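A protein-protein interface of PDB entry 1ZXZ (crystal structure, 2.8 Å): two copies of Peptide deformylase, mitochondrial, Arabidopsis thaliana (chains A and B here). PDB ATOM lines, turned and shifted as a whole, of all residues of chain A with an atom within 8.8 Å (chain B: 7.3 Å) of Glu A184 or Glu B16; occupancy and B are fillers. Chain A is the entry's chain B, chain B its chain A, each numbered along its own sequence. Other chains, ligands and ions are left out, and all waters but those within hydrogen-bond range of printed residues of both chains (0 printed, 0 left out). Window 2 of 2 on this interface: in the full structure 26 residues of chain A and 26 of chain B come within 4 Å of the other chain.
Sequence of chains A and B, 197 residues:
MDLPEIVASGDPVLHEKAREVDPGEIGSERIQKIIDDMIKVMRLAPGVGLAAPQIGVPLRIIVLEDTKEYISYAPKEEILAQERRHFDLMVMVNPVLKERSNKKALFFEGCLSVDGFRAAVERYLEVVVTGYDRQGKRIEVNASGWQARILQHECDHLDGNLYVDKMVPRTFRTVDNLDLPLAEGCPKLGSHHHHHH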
ATOM      1  N   PRO A 169      28.904 -23.302  -4.977  1.00  0.00           N
ATOM      2  CA  PRO A 169      28.507 -21.969  -4.529  1.00  0.00           C
ATOM      3  C   PRO A 169      27.012 -21.834  -4.264  1.00  0.00           C
ATOM      4  O   PRO A 169      26.190 -22.237  -5.072  1.00  0.00           O
ATOM      5  CB  PRO A 169      28.977 -21.083  -5.671  1.00  0.00           C
ATOM      6  CG  PRO A 169      30.192 -21.793  -6.148  1.00  0.00           C
ATOM      7  CD  PRO A 169      29.722 -23.218  -6.196  1.00  0.00           C
ATOM      8  N   ARG A 170      26.669 -21.247  -3.127  1.00  0.00           N
ATOM      9  CA  ARG A 170      25.275 -21.047  -2.720  1.00  0.00           C
ATOM     10  C   ARG A 170      24.332 -22.241  -2.780  1.00  0.00           C
ATOM     11  O   ARG A 170      23.268 -22.191  -3.404  1.00  0.00           O
ATOM     12  CB  ARG A 170      24.643 -19.872  -3.472  1.00  0.00           C
ATOM     13  CG  ARG A 170      24.943 -19.763  -4.928  1.00  0.00           C
ATOM     14  CD  ARG A 170      24.901 -18.289  -5.260  1.00  0.00           C
ATOM     15  NE  ARG A 170      25.331 -17.983  -6.616  1.00  0.00           N
ATOM     16  CZ  ARG A 170      25.678 -16.769  -7.025  1.00  0.00           C
ATOM     17  NH1 ARG A 170      25.650 -15.749  -6.182  1.00  0.00           N
ATOM     18  NH2 ARG A 170      26.038 -16.575  -8.284  1.00  0.00           N
ATOM     19  N   ARG A 173      23.403 -24.826   3.068  1.00  0.00           N
ATOM     20  CA  ARG A 173      22.188 -24.495   3.775  1.00  0.00           C
ATOM     21  C   ARG A 173      21.967 -25.182   5.110  1.00  0.00           C
ATOM     22  O   ARG A 173      22.643 -26.143   5.490  1.00  0.00           O
ATOM     23  CB  ARG A 173      21.001 -24.790   2.876  1.00  0.00           C
ATOM     24  CG  ARG A 173      20.882 -26.249   2.542  1.00  0.00           C
ATOM     25  CD  ARG A 173      19.943 -26.440   1.375  1.00  0.00           C
ATOM     26  NE  ARG A 173      20.399 -25.704   0.195  1.00  0.00           N
ATOM     27  CZ  ARG A 173      19.651 -25.493  -0.882  1.00  0.00           C
ATOM     28  NH1 ARG A 173      18.412 -25.953  -0.927  1.00  0.00           N
ATOM     29  NH2 ARG A 173      20.150 -24.842  -1.923  1.00  0.00           N
ATOM     30  N   PRO A 181      14.522 -24.953  -2.729  1.00  0.00           N
ATOM     31  CA  PRO A 181      15.077 -24.892  -4.088  1.00  0.00           C
ATOM     32  C   PRO A 181      16.528 -24.433  -4.235  1.00  0.00           C
ATOM     33  O   PRO A 181      17.034 -23.615  -3.459  1.00  0.00           O
ATOM     34  CB  PRO A 181      14.122 -23.942  -4.816  1.00  0.00           C
ATOM     35  CG  PRO A 181      12.862 -24.013  -4.017  1.00  0.00           C
ATOM     36  CD  PRO A 181      13.365 -24.053  -2.604  1.00  0.00           C
ATOM     37  N   LEU A 182      17.192 -24.978  -5.247  1.00  0.00           N
ATOM     38  CA  LEU A 182      18.561 -24.593  -5.540  1.00  0.00           C
ATOM     39  C   LEU A 182      18.405 -23.239  -6.204  1.00  0.00           C
ATOM     40  O   LEU A 182      17.416 -22.998  -6.888  1.00  0.00           O
ATOM     41  CB  LEU A 182      19.204 -25.600  -6.496  1.00  0.00           C
ATOM     42  CG  LEU A 182      19.751 -26.855  -5.818  1.00  0.00           C
ATOM     43  CD1 LEU A 182      19.329 -28.082  -6.573  1.00  0.00           C
ATOM     44  CD2 LEU A 182      21.259 -26.757  -5.738  1.00  0.00           C
ATOM     45  N   ALA A 183      19.365 -22.351  -5.990  1.00  0.00           N
ATOM     46  CA  ALA A 183      19.298 -21.013  -6.561  1.00  0.00           C
ATOM     47  C   ALA A 183      19.551 -20.964  -8.067  1.00  0.00           C
ATOM     48  O   ALA A 183      20.257 -21.805  -8.623  1.00  0.00           O
ATOM     49  CB  ALA A 183      20.276 -20.107  -5.845  1.00  0.00           C
ATOM     50  N   GLU A 184      18.966 -19.961  -8.714  1.00  0.00           N
ATOM     51  CA  GLU A 184      19.109 -19.779 -10.152  1.00  0.00           C
ATOM     52  C   GLU A 184      20.579 -19.603 -10.472  1.00  0.00           C
ATOM     53  O   GLU A 184      21.215 -18.671  -9.991  1.00  0.00           O
ATOM     54  CB  GLU A 184      18.318 -18.554 -10.612  1.00  0.00           C
ATOM     55  N   GLY A 185      21.111 -20.505 -11.288  1.00  0.00           N
ATOM     56  CA  GLY A 185      22.516 -20.443 -11.643  1.00  0.00           C
ATOM     57  C   GLY A 185      23.249 -21.661 -11.115  1.00  0.00           C
ATOM     58  O   GLY A 185      24.396 -21.920 -11.479  1.00  0.00           O
ATOM     59  N   CYS A 186      22.576 -22.413 -10.252  1.00  0.00           N
ATOM     60  CA  CYS A 186      23.161 -23.614  -9.672  1.00  0.00           C
ATOM     61  C   CYS A 186      22.983 -24.799 -10.598  1.00  0.00           C
ATOM     62  O   CYS A 186      22.023 -24.864 -11.362  1.00  0.00           O
ATOM     63  CB  CYS A 186      22.501 -23.942  -8.330  1.00  0.00           C
ATOM     64  SG  CYS A 186      22.912 -22.811  -6.998  1.00  0.00           S
ATOM     65  N   PRO A 187      23.930 -25.744 -10.565  1.00  0.00           N
ATOM     66  CA  PRO A 187      23.811 -26.924 -11.423  1.00  0.00           C
ATOM     67  C   PRO A 187      22.626 -27.699 -10.854  1.00  0.00           C
ATOM     68  O   PRO A 187      21.958 -27.230  -9.932  1.00  0.00           O
ATOM     69  CB  PRO A 187      25.130 -27.651 -11.188  1.00  0.00           C
ATOM     70  CG  PRO A 187      26.085 -26.531 -10.819  1.00  0.00           C
ATOM     71  CD  PRO A 187      25.240 -25.705  -9.893  1.00  0.00           C
ATOM     72  N   ASP B  11      17.183 -20.561   1.722  1.00  0.00           N
ATOM     73  CA  ASP B  11      16.130 -19.759   1.108  1.00  0.00           C
ATOM     74  C   ASP B  11      16.752 -18.983  -0.062  1.00  0.00           C
ATOM     75  O   ASP B  11      17.673 -18.189   0.134  1.00  0.00           O
ATOM     76  CB  ASP B  11      15.546 -18.789   2.132  1.00  0.00           C
ATOM     77  CG  ASP B  11      14.104 -18.450   1.846  1.00  0.00           C
ATOM     78  OD1 ASP B  11      13.813 -17.918   0.748  1.00  0.00           O
ATOM     79  OD2 ASP B  11      13.262 -18.721   2.727  1.00  0.00           O
ATOM     80  N   PRO B  12      16.244 -19.203  -1.290  1.00  0.00           N
ATOM     81  CA  PRO B  12      16.702 -18.574  -2.536  1.00  0.00           C
ATOM     82  C   PRO B  12      16.937 -17.063  -2.531  1.00  0.00           C
ATOM     83  O   PRO B  12      17.873 -16.579  -3.176  1.00  0.00           O
ATOM     84  CB  PRO B  12      15.625 -18.986  -3.539  1.00  0.00           C
ATOM     85  CG  PRO B  12      15.215 -20.331  -3.040  1.00  0.00           C
ATOM     86  CD  PRO B  12      15.093 -20.084  -1.556  1.00  0.00           C
ATOM     87  N   VAL B  13      16.087 -16.320  -1.822  1.00  0.00           N
ATOM     88  CA  VAL B  13      16.220 -14.865  -1.773  1.00  0.00           C
ATOM     89  C   VAL B  13      17.587 -14.478  -1.197  1.00  0.00           C
ATOM     90  O   VAL B  13      18.039 -13.338  -1.319  1.00  0.00           O
ATOM     91  CB  VAL B  13      15.104 -14.226  -0.906  1.00  0.00           C
ATOM     92  CG1 VAL B  13      15.330 -14.543   0.569  1.00  0.00           C
ATOM     93  CG2 VAL B  13      15.065 -12.734  -1.134  1.00  0.00           C
ATOM     94  N   LEU B  14      18.245 -15.449  -0.577  1.00  0.00           N
ATOM     95  CA  LEU B  14      19.543 -15.231   0.027  1.00  0.00           C
ATOM     96  C   LEU B  14      20.643 -15.496  -0.991  1.00  0.00           C
ATOM     97  O   LEU B  14      21.726 -14.918  -0.908  1.00  0.00           O
ATOM     98  CB  LEU B  14      19.690 -16.169   1.230  1.00  0.00           C
ATOM     99  CG  LEU B  14      20.059 -15.609   2.608  1.00  0.00           C
ATOM    100  CD1 LEU B  14      19.287 -14.345   2.911  1.00  0.00           C
ATOM    101  CD2 LEU B  14      19.768 -16.664   3.652  1.00  0.00           C
ATOM    102  N   HIS B  15      20.350 -16.359  -1.963  1.00  0.00           N
ATOM    103  CA  HIS B  15      21.323 -16.740  -2.991  1.00  0.00           C
ATOM    104  C   HIS B  15      20.974 -16.262  -4.390  1.00  0.00           C
ATOM    105  O   HIS B  15      21.516 -16.774  -5.375  1.00  0.00           O
ATOM    106  CB  HIS B  15      21.491 -18.261  -3.010  1.00  0.00           C
ATOM    107  CG  HIS B  15      21.535 -18.876  -1.645  1.00  0.00           C
ATOM    108  ND1 HIS B  15      20.437 -18.912  -0.817  1.00  0.00           N
ATOM    109  CD2 HIS B  15      22.554 -19.426  -0.946  1.00  0.00           C
ATOM    110  CE1 HIS B  15      20.777 -19.456   0.339  1.00  0.00           C
ATOM    111  NE2 HIS B  15      22.054 -19.776   0.287  1.00  0.00           N
ATOM    112  N   GLU B  16      20.075 -15.284  -4.476  1.00  0.00           N
ATOM    113  CA  GLU B  16      19.663 -14.719  -5.760  1.00  0.00           C
ATOM    114  C   GLU B  16      19.803 -13.194  -5.745  1.00  0.00           C
ATOM    115  O   GLU B  16      19.581 -12.550  -4.726  1.00  0.00           O
ATOM    116  CB  GLU B  16      18.225 -15.146  -6.077  1.00  0.00           C
ATOM    117  CG  GLU B  16      18.125 -16.589  -6.584  1.00  0.00           C
ATOM    118  CD  GLU B  16      16.716 -17.155  -6.533  1.00  0.00           C
ATOM    119  OE1 GLU B  16      15.751 -16.364  -6.506  1.00  0.00           O
ATOM    120  OE2 GLU B  16      16.572 -18.398  -6.533  1.00  0.00           O
ATOM    121  N   LYS B  17      20.189 -12.625  -6.876  1.00  0.00           N
ATOM    122  CA  LYS B  17      20.401 -11.187  -7.008  1.00  0.00           C
ATOM    123  C   LYS B  17      19.185 -10.328  -6.658  1.00  0.00           C
ATOM    124  O   LYS B  17      18.098 -10.547  -7.174  1.00  0.00           O
ATOM    125  CB  LYS B  17      20.847 -10.887  -8.434  1.00  0.00           C
ATOM    126  CG  LYS B  17      21.387  -9.494  -8.642  1.00  0.00           C
ATOM    127  CD  LYS B  17      22.121  -9.409  -9.967  1.00  0.00           C
ATOM    128  CE  LYS B  17      22.874  -8.098 -10.113  1.00  0.00           C
ATOM    129  NZ  LYS B  17      23.804  -8.172 -11.272  1.00  0.00           N
ATOM    130  N   ALA B  18      19.386  -9.332  -5.802  1.00  0.00           N
ATOM    131  CA  ALA B  18      18.308  -8.447  -5.370  1.00  0.00           C
ATOM    132  C   ALA B  18      18.142  -7.264  -6.312  1.00  0.00           C
ATOM    133  O   ALA B  18      19.102  -6.555  -6.606  1.00  0.00           O
ATOM    134  CB  ALA B  18      18.587  -7.953  -3.955  1.00  0.00           C
ATOM    135  N   ARG B  19      16.914  -7.046  -6.768  1.00  0.00           N
ATOM    136  CA  ARG B  19      16.617  -5.952  -7.687  1.00  0.00           C
ATOM    137  C   ARG B  19      16.474  -4.578  -7.034  1.00  0.00           C
ATOM    138  O   ARG B  19      16.086  -4.466  -5.872  1.00  0.00           O
ATOM    139  CB  ARG B  19      15.389  -6.312  -8.535  1.00  0.00           C
ATOM    140  CG  ARG B  19      15.787  -7.040  -9.826  1.00  0.00           C
ATOM    141  CD  ARG B  19      14.615  -7.495 -10.630  1.00  0.00           C
ATOM    142  NE  ARG B  19      14.210  -8.896 -10.272  1.00  0.00           N
ATOM    143  CZ  ARG B  19      13.421  -9.702 -10.968  1.00  0.00           C
ATOM    144  NH1 ARG B  19      12.892  -9.249 -12.077  1.00  0.00           N
ATOM    145  NH2 ARG B  19      13.132 -10.943 -10.583  1.00  0.00           N
ATOM    146  N   PRO B  53      17.473  -8.940   1.674  1.00  0.00           N
ATOM    147  CA  PRO B  53      17.227 -10.370   1.486  1.00  0.00           C
ATOM    148  C   PRO B  53      17.190 -11.126   2.800  1.00  0.00           C
ATOM    149  O   PRO B  53      16.447 -12.095   2.934  1.00  0.00           O
ATOM    150  CB  PRO B  53      18.393 -10.802   0.617  1.00  0.00           C
ATOM    151  CG  PRO B  53      18.597  -9.621  -0.243  1.00  0.00           C
ATOM    152  CD  PRO B  53      18.500  -8.468   0.732  1.00  0.00           C
ATOM    153  N   PRO B  58      13.644  -9.028  -1.398  1.00  0.00           N
ATOM    154  CA  PRO B  58      14.452  -9.053  -2.622  1.00  0.00           C
ATOM    155  C   PRO B  58      14.838  -7.696  -3.216  1.00  0.00           C
ATOM    156  O   PRO B  58      14.867  -7.537  -4.438  1.00  0.00           O
ATOM    157  CB  PRO B  58      13.585  -9.870  -3.576  1.00  0.00           C
ATOM    158  CG  PRO B  58      12.206  -9.433  -3.200  1.00  0.00           C
ATOM    159  CD  PRO B  58      12.263  -9.467  -1.678  1.00  0.00           C
ATOM    160  N   ASP B 156      27.452  -7.795  -0.729  1.00  0.00           N
ATOM    161  CA  ASP B 156      27.534  -9.133  -1.301  1.00  0.00           C
ATOM    162  C   ASP B 156      26.151  -9.764  -1.241  1.00  0.00           C
ATOM    163  O   ASP B 156      25.665 -10.326  -2.221  1.00  0.00           O
ATOM    164  CB  ASP B 156      28.526  -9.982  -0.517  1.00  0.00           C
ATOM    165  CG  ASP B 156      29.952  -9.720  -0.925  1.00  0.00           C
ATOM    166  OD1 ASP B 156      30.194  -8.658  -1.528  1.00  0.00           O
ATOM    167  OD2 ASP B 156      30.833 -10.561  -0.643  1.00  0.00           O
ATOM    168  N   HIS B 157      25.523  -9.661  -0.076  1.00  0.00           N
ATOM    169  CA  HIS B 157      24.188 -10.197   0.118  1.00  0.00           C
ATOM    170  C   HIS B 157      23.248  -9.786  -1.017  1.00  0.00           C
ATOM    171  O   HIS B 157      22.415 -10.578  -1.457  1.00  0.00           O
ATOM    172  CB  HIS B 157      23.621  -9.698   1.442  1.00  0.00           C
ATOM    173  CG  HIS B 157      23.972 -10.554   2.616  1.00  0.00           C
ATOM    174  ND1 HIS B 157      23.514 -11.845   2.753  1.00  0.00           N
ATOM    175  CD2 HIS B 157      24.721 -10.301   3.709  1.00  0.00           C
ATOM    176  CE1 HIS B 157      23.968 -12.351   3.884  1.00  0.00           C
ATOM    177  NE2 HIS B 157      24.703 -11.437   4.483  1.00  0.00           N
ATOM    178  N   LEU B 158      23.382  -8.550  -1.492  1.00  0.00           N
ATOM    179  CA  LEU B 158      22.522  -8.050  -2.564  1.00  0.00           C
ATOM    180  C   LEU B 158      22.721  -8.740  -3.908  1.00  0.00           C
ATOM    181  O   LEU B 158      21.898  -8.600  -4.814  1.00  0.00           O
ATOM    182  CB  LEU B 158      22.710  -6.545  -2.732  1.00  0.00           C
ATOM    183  CG  LEU B 158      22.297  -5.718  -1.520  1.00  0.00           C
ATOM    184  CD1 LEU B 158      22.386  -4.241  -1.873  1.00  0.00           C
ATOM    185  CD2 LEU B 158      20.879  -6.092  -1.108  1.00  0.00           C
ATOM    186  N   ASP B 159      23.818  -9.469  -4.048  1.00  0.00           N
ATOM    187  CA  ASP B 159      24.070 -10.182  -5.282  1.00  0.00           C
ATOM    188  C   ASP B 159      23.999 -11.689  -5.034  1.00  0.00           C
ATOM    189  O   ASP B 159      24.467 -12.482  -5.852  1.00  0.00           O
ATOM    190  CB  ASP B 159      25.432  -9.798  -5.853  1.00  0.00           C
ATOM    191  CG  ASP B 159      25.345  -8.655  -6.853  1.00  0.00           C
ATOM    192  OD1 ASP B 159      24.536  -8.764  -7.800  1.00  0.00           O
ATOM    193  OD2 ASP B 159      26.084  -7.657  -6.706  1.00  0.00           O
ATOM    194  N   GLY B 160      23.407 -12.071  -3.901  1.00  0.00           N
ATOM    195  CA  GLY B 160      23.258 -13.476  -3.543  1.00  0.00           C
ATOM    196  C   GLY B 160      24.518 -14.237  -3.151  1.00  0.00           C
ATOM    197  O   GLY B 160      24.599 -15.449  -3.361  1.00  0.00           O
ATOM    198  N   ASN B 161      25.493 -13.543  -2.570  1.00  0.00           N
ATOM    199  CA  ASN B 161      26.742 -14.176  -2.156  1.00  0.00           C
ATOM    200  C   ASN B 161      26.940 -14.144  -0.647  1.00  0.00           C
ATOM    201  O   ASN B 161      26.678 -13.128  -0.008  1.00  0.00           O
ATOM    202  CB  ASN B 161      27.907 -13.472  -2.823  1.00  0.00           C
ATOM    203  CG  ASN B 161      27.645 -13.214  -4.271  1.00  0.00           C
ATOM    204  OD1 ASN B 161      27.239 -14.117  -4.998  1.00  0.00           O
ATOM    205  ND2 ASN B 161      27.865 -11.977  -4.710  1.00  0.00           N
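The guanidinium group of Arg A170 lies within hydrogen-bond range of the backbone carbonyl oxygen of Gly B160 (3.0 Å). The side-chain amide oxygen (OD1) of Asn B161 is in hydrogen-bond range of the guanidinium group (NH1) of Arg A170 (2.6 Å). O of Asp B159 lies within hydrogen-bond range of NH1 of Arg A170, at 3.5 Å.
The backbone carbonyl oxygen of Asp B156 sits at hydrogen-bond distance from the backbone NH of Asn B161. The side-chain carboxylate of Asp B159 lies within salt-bridge range of the side-chain amino group of Lys B17, 3.6 Å away. The backbone carbonyl oxygen (O) of Arg A170 sits at hydrogen-bond distance from the side-chain sulfur (SG) of Cys A186 (3.7 Å). OD1 of Asn B161 lies close to O of Asp B159 (3.3 Å). The backbone carbonyl oxygen of Ala A183 lies close to the side-chain sulfur of Cys A186, at 3.3 Å. O of Asp B11 lies within hydrogen-bond range of ND1 of His B15 (3.0 Å).
CD2 of His B15 touches CB of Arg A170, at 3.3 Å. O of Pro A181 touches CG of Pro B12, 3.8 Å away. Ala A183 touches His B15 (CB to O, 3.6 Å). Ala A183 touches Glu B16 (CA to OE2, 3.8 Å). Glu B16 touches Glu A184 (OE2 to N, 3.6 Å).
Of chain B, only Glu B16 (3.6 Å) comes within 4 Å of Glu A184. Glu B16 touches two residues of chain A. Of the printed residues of chain B, Pro A181 touches Pro B12. Of the printed residues of chain A, Gly B160 touches Arg A170 (3.0 Å). Of the printed residues of chain B, Arg A170 touches His B15, Asp B159, Gly B160 and Asn B161. Of the printed residues of chain A, Asp B159 touches Arg A170 (3.5 Å). Leu B158 touches none of the printed residues of chain A. The nearest printed residue of chain A that does not touch His B15 is Glu A184 (5.0 Å).
Along chain A the printed residues that touch a printed residue of chain B span positions 170 to 184. Of the 17 printed residues of chain B, 6 touch a printed residue of chain A. Hydrophobic or aromatic side chains of chain B that line the printed part of chain A: Pro B12 and His B15. Among the printed residues, no Asp or Glu carboxylate lies within 4 Å of a Lys or Arg side-chain nitrogen of the other chain.
No position is printed for both chains. Of the 8 pairs that touch across the chains among the printed residues, none has its exchanged pair printed and touching as well.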
